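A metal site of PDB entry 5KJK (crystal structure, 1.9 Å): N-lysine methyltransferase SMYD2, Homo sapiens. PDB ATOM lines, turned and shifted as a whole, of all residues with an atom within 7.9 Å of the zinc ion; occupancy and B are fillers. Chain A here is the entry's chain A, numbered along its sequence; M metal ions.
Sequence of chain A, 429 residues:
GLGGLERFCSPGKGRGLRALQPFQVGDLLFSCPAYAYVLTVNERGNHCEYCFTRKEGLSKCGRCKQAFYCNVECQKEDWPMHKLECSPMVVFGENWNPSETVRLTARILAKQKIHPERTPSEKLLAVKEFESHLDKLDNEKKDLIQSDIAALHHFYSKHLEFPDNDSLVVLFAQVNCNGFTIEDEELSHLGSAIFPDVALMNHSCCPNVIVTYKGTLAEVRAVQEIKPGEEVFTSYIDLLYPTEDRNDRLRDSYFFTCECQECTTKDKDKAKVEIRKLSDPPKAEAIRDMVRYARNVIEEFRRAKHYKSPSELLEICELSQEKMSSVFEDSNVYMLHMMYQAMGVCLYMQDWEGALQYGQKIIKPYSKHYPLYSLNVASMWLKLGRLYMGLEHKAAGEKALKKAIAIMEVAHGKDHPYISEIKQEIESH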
ATOM      1  N   HIS A  47      23.119   3.457 -15.227  1.00  0.00           N
ATOM      2  CA  HIS A  47      24.004   3.344 -14.080  1.00  0.00           C
ATOM      3  C   HIS A  47      23.178   3.200 -12.848  1.00  0.00           C
ATOM      4  O   HIS A  47      22.087   3.773 -12.744  1.00  0.00           O
ATOM      5  CB  HIS A  47      24.870   4.594 -13.931  1.00  0.00           C
ATOM      6  CG  HIS A  47      25.851   4.827 -15.022  1.00  0.00           C
ATOM      7  ND1 HIS A  47      27.209   4.593 -14.838  1.00  0.00           N
ATOM      8  CD2 HIS A  47      25.655   5.281 -16.276  1.00  0.00           C
ATOM      9  CE1 HIS A  47      27.790   4.911 -15.982  1.00  0.00           C
ATOM     10  NE2 HIS A  47      26.894   5.313 -16.887  1.00  0.00           N
ATOM     11  N   CYS A  48      23.716   2.464 -11.876  1.00  0.00           N
ATOM     12  CA  CYS A  48      23.094   2.332 -10.576  1.00  0.00           C
ATOM     13  C   CYS A  48      23.191   3.682  -9.848  1.00  0.00           C
ATOM     14  O   CYS A  48      24.253   4.293  -9.771  1.00  0.00           O
ATOM     15  CB  CYS A  48      23.767   1.218  -9.787  1.00  0.00           C
ATOM     16  SG  CYS A  48      23.269   1.176  -8.050  1.00  0.00           S
ATOM     17  N   GLU A  49      22.069   4.113  -9.290  1.00  0.00           N
ATOM     18  CA  GLU A  49      21.869   5.341  -8.537  1.00  0.00           C
ATOM     19  C   GLU A  49      22.862   5.375  -7.348  1.00  0.00           C
ATOM     20  O   GLU A  49      23.494   6.399  -7.100  1.00  0.00           O
ATOM     21  CB  GLU A  49      20.410   5.243  -8.008  1.00  0.00           C
ATOM     22  CG  GLU A  49      19.469   6.410  -8.091  1.00  0.00           C
ATOM     23  CD  GLU A  49      19.266   7.184  -9.375  1.00  0.00           C
ATOM     24  OE1 GLU A  49      18.965   6.612 -10.438  1.00  0.00           O
ATOM     25  OE2 GLU A  49      19.297   8.427  -9.249  1.00  0.00           O
ATOM     26  N   TYR A  50      23.013   4.238  -6.629  1.00  0.00           N
ATOM     27  CA  TYR A  50      23.836   4.168  -5.416  1.00  0.00           C
ATOM     28  C   TYR A  50      25.344   4.122  -5.636  1.00  0.00           C
ATOM     29  O   TYR A  50      26.063   4.903  -5.009  1.00  0.00           O
ATOM     30  CB  TYR A  50      23.408   3.016  -4.489  1.00  0.00           C
ATOM     31  CG  TYR A  50      24.222   2.951  -3.218  1.00  0.00           C
ATOM     32  CD1 TYR A  50      25.119   1.918  -2.981  1.00  0.00           C
ATOM     33  CD2 TYR A  50      24.121   3.960  -2.251  1.00  0.00           C
ATOM     34  CE1 TYR A  50      25.894   1.872  -1.825  1.00  0.00           C
ATOM     35  CE2 TYR A  50      24.908   3.949  -1.102  1.00  0.00           C
ATOM     36  CZ  TYR A  50      25.799   2.896  -0.900  1.00  0.00           C
ATOM     37  OH  TYR A  50      26.556   2.857   0.244  1.00  0.00           O
ATOM     38  N   CYS A  51      25.817   3.201  -6.489  1.00  0.00           N
ATOM     39  CA  CYS A  51      27.249   2.991  -6.692  1.00  0.00           C
ATOM     40  C   CYS A  51      27.790   3.420  -8.084  1.00  0.00           C
ATOM     41  O   CYS A  51      28.993   3.324  -8.317  1.00  0.00           O
ATOM     42  CB  CYS A  51      27.567   1.532  -6.400  1.00  0.00           C
ATOM     43  SG  CYS A  51      26.980   0.405  -7.678  1.00  0.00           S
ATOM     44  N   PHE A  52      26.902   3.875  -8.995  1.00  0.00           N
ATOM     45  CA  PHE A  52      27.240   4.338 -10.366  1.00  0.00           C
ATOM     46  C   PHE A  52      27.763   3.229 -11.305  1.00  0.00           C
ATOM     47  O   PHE A  52      28.299   3.531 -12.373  1.00  0.00           O
ATOM     48  CB  PHE A  52      28.207   5.550 -10.366  1.00  0.00           C
ATOM     49  CG  PHE A  52      27.654   6.941 -10.176  1.00  0.00           C
ATOM     50  CD1 PHE A  52      28.256   8.040 -10.791  1.00  0.00           C
ATOM     51  CD2 PHE A  52      26.506   7.156  -9.409  1.00  0.00           C
ATOM     52  CE1 PHE A  52      27.764   9.332 -10.590  1.00  0.00           C
ATOM     53  CE2 PHE A  52      26.028   8.461  -9.195  1.00  0.00           C
ATOM     54  CZ  PHE A  52      26.669   9.535  -9.774  1.00  0.00           C
ATOM     55  N   THR A  53      27.578   1.946 -10.942  1.00  0.00           N
ATOM     56  CA  THR A  53      27.989   0.804 -11.782  1.00  0.00           C
ATOM     57  C   THR A  53      27.166   0.847 -13.054  1.00  0.00           C
ATOM     58  O   THR A  53      25.954   0.993 -12.981  1.00  0.00           O
ATOM     59  CB  THR A  53      27.814  -0.535 -11.017  1.00  0.00           C
ATOM     60  OG1 THR A  53      28.747  -0.549  -9.936  1.00  0.00           O
ATOM     61  CG2 THR A  53      28.020  -1.785 -11.886  1.00  0.00           C
ATOM     62  N   ARG A  54      27.825   0.803 -14.215  1.00  0.00           N
ATOM     63  CA  ARG A  54      27.157   0.770 -15.502  1.00  0.00           C
ATOM     64  C   ARG A  54      26.924  -0.724 -15.806  1.00  0.00           C
ATOM     65  O   ARG A  54      27.868  -1.519 -15.871  1.00  0.00           O
ATOM     66  CB  ARG A  54      28.005   1.452 -16.558  1.00  0.00           C
ATOM     67  CG  ARG A  54      27.352   1.500 -17.929  1.00  0.00           C
ATOM     68  CD  ARG A  54      28.206   2.321 -18.894  1.00  0.00           C
ATOM     69  NE  ARG A  54      29.553   1.781 -19.064  1.00  0.00           N
ATOM     70  CZ  ARG A  54      30.639   2.530 -19.256  1.00  0.00           C
ATOM     71  NH1 ARG A  54      30.529   3.846 -19.309  1.00  0.00           N
ATOM     72  NH2 ARG A  54      31.825   1.962 -19.414  1.00  0.00           N
ATOM     73  N   LYS A  55      25.634  -1.108 -15.923  1.00  0.00           N
ATOM     74  CA  LYS A  55      25.205  -2.503 -16.069  1.00  0.00           C
ATOM     75  C   LYS A  55      23.871  -2.575 -16.810  1.00  0.00           C
ATOM     76  O   LYS A  55      23.096  -1.624 -16.795  1.00  0.00           O
ATOM     77  CB  LYS A  55      24.996  -3.074 -14.640  1.00  0.00           C
ATOM     78  CG  LYS A  55      25.146  -4.564 -14.470  1.00  0.00           C
ATOM     79  CD  LYS A  55      24.819  -4.946 -13.033  1.00  0.00           C
ATOM     80  CE  LYS A  55      23.780  -6.046 -12.969  1.00  0.00           C
ATOM     81  NZ  LYS A  55      23.192  -6.165 -11.601  1.00  0.00           N
ATOM     82  N   LEU A  58      19.481  -3.492 -14.591  1.00  0.00           N
ATOM     83  CA  LEU A  58      19.372  -2.762 -13.328  1.00  0.00           C
ATOM     84  C   LEU A  58      17.885  -2.775 -12.927  1.00  0.00           C
ATOM     85  O   LEU A  58      17.017  -2.627 -13.797  1.00  0.00           O
ATOM     86  CB  LEU A  58      19.872  -1.310 -13.459  1.00  0.00           C
ATOM     87  CG  LEU A  58      21.386  -1.099 -13.662  1.00  0.00           C
ATOM     88  CD1 LEU A  58      21.664   0.325 -14.124  1.00  0.00           C
ATOM     89  CD2 LEU A  58      22.182  -1.364 -12.390  1.00  0.00           C
ATOM     90  N   PHE A  68      17.207   3.423 -10.683  1.00  0.00           N
ATOM     91  CA  PHE A  68      17.613   2.050 -11.033  1.00  0.00           C
ATOM     92  C   PHE A  68      18.806   1.652 -10.208  1.00  0.00           C
ATOM     93  O   PHE A  68      19.691   2.477  -9.957  1.00  0.00           O
ATOM     94  CB  PHE A  68      17.881   1.910 -12.542  1.00  0.00           C
ATOM     95  CG  PHE A  68      16.690   2.241 -13.420  1.00  0.00           C
ATOM     96  CD1 PHE A  68      15.970   1.222 -14.042  1.00  0.00           C
ATOM     97  CD2 PHE A  68      16.311   3.558 -13.653  1.00  0.00           C
ATOM     98  CE1 PHE A  68      14.885   1.533 -14.870  1.00  0.00           C
ATOM     99  CE2 PHE A  68      15.222   3.857 -14.474  1.00  0.00           C
ATOM    100  CZ  PHE A  68      14.523   2.844 -15.091  1.00  0.00           C
ATOM    101  N   TYR A  69      18.811   0.377  -9.776  1.00  0.00           N
ATOM    102  CA  TYR A  69      19.824  -0.181  -8.885  1.00  0.00           C
ATOM    103  C   TYR A  69      20.373  -1.516  -9.308  1.00  0.00           C
ATOM    104  O   TYR A  69      19.705  -2.235 -10.060  1.00  0.00           O
ATOM    105  CB  TYR A  69      19.220  -0.338  -7.474  1.00  0.00           C
ATOM    106  CG  TYR A  69      18.728   0.980  -6.909  1.00  0.00           C
ATOM    107  CD1 TYR A  69      17.377   1.317  -6.946  1.00  0.00           C
ATOM    108  CD2 TYR A  69      19.625   1.913  -6.391  1.00  0.00           C
ATOM    109  CE1 TYR A  69      16.930   2.537  -6.448  1.00  0.00           C
ATOM    110  CE2 TYR A  69      19.186   3.112  -5.866  1.00  0.00           C
ATOM    111  CZ  TYR A  69      17.839   3.430  -5.905  1.00  0.00           C
ATOM    112  OH  TYR A  69      17.420   4.634  -5.389  1.00  0.00           O
ATOM    113  N   CYS A  70      21.571  -1.871  -8.803  1.00  0.00           N
ATOM    114  CA  CYS A  70      22.213  -3.175  -9.059  1.00  0.00           C
ATOM    115  C   CYS A  70      21.332  -4.294  -8.495  1.00  0.00           C
ATOM    116  O   CYS A  70      21.201  -5.361  -9.114  1.00  0.00           O
ATOM    117  CB  CYS A  70      23.589  -3.231  -8.407  1.00  0.00           C
ATOM    118  SG  CYS A  70      24.803  -2.125  -9.156  1.00  0.00           S
ATOM    119  N   ASN A  71      20.838  -4.083  -7.268  1.00  0.00           N
ATOM    120  CA  ASN A  71      20.076  -5.036  -6.470  1.00  0.00           C
ATOM    121  C   ASN A  71      19.366  -4.303  -5.331  1.00  0.00           C
ATOM    122  O   ASN A  71      19.445  -3.066  -5.247  1.00  0.00           O
ATOM    123  CB  ASN A  71      21.041  -6.088  -5.878  1.00  0.00           C
ATOM    124  CG  ASN A  71      22.318  -5.502  -5.323  1.00  0.00           C
ATOM    125  OD1 ASN A  71      22.319  -4.670  -4.412  1.00  0.00           O
ATOM    126  ND2 ASN A  71      23.449  -5.910  -5.882  1.00  0.00           N
ATOM    127  N   GLU A  73      20.255  -4.226  -2.172  1.00  0.00           N
ATOM    128  CA  GLU A  73      21.213  -3.574  -1.267  1.00  0.00           C
ATOM    129  C   GLU A  73      21.511  -2.166  -1.718  1.00  0.00           C
ATOM    130  O   GLU A  73      21.420  -1.267  -0.899  1.00  0.00           O
ATOM    131  CB  GLU A  73      22.517  -4.384  -1.101  1.00  0.00           C
ATOM    132  CG  GLU A  73      22.556  -5.246   0.164  1.00  0.00           C
ATOM    133  CD  GLU A  73      21.303  -6.023   0.503  1.00  0.00           C
ATOM    134  OE1 GLU A  73      20.696  -5.724   1.562  1.00  0.00           O
ATOM    135  OE2 GLU A  73      20.909  -6.902  -0.296  1.00  0.00           O
ATOM    136  N   CYS A  74      21.848  -1.975  -3.029  1.00  0.00           N
ATOM    137  CA  CYS A  74      22.085  -0.646  -3.596  1.00  0.00           C
ATOM    138  C   CYS A  74      20.798   0.205  -3.407  1.00  0.00           C
ATOM    139  O   CYS A  74      20.876   1.332  -2.928  1.00  0.00           O
ATOM    140  CB  CYS A  74      22.514  -0.732  -5.059  1.00  0.00           C
ATOM    141  SG  CYS A  74      24.272  -1.192  -5.306  1.00  0.00           S
ATOM    142  N   GLN A  75      19.612  -0.380  -3.674  1.00  0.00           N
ATOM    143  CA  GLN A  75      18.329   0.306  -3.470  1.00  0.00           C
ATOM    144  C   GLN A  75      18.161   0.815  -2.037  1.00  0.00           C
ATOM    145  O   GLN A  75      17.877   2.001  -1.846  1.00  0.00           O
ATOM    146  CB  GLN A  75      17.145  -0.598  -3.879  1.00  0.00           C
ATOM    147  CG  GLN A  75      15.797   0.135  -3.829  1.00  0.00           C
ATOM    148  CD  GLN A  75      14.628  -0.584  -4.475  1.00  0.00           C
ATOM    149  OE1 GLN A  75      13.508  -0.067  -4.548  1.00  0.00           O
ATOM    150  NE2 GLN A  75      14.837  -1.812  -4.901  1.00  0.00           N
HETATM  151 ZN    ZN M   1      24.799  -0.433  -7.331  1.00  0.00          ZN
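N of Cys 74 lies within hydrogen-bond range of OD1 of Asn 71 (3.1 Å).
The side-chain amino group (NZ) of Lys 55 is in hydrogen-bond range of the backbone carbonyl oxygen (O) of Cys 70, 3.3 Å away.
The backbone NH (N) of Tyr 50 sits close to the side-chain sulfur (SG) of Cys 48, 3.4 Å away.
The backbone NH (N) of Cys 48 is in hydrogen-bond range of the backbone carbonyl oxygen (O) of Thr 53, 2.9 Å away.
SG of Cys 51 sits close to OG1 of Thr 53.
The nearest printed residue that does not touch the zinc ion is Tyr 50 (4.7 Å).
The zinc ion is bound by SG of Cys 74 (2.2 Å), SG of Cys 48 (2.3 Å), SG of Cys 51 (2.4 Å) and SG of Cys 70 (2.5 Å).
The zinc ion has four donor atoms within binding distance.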
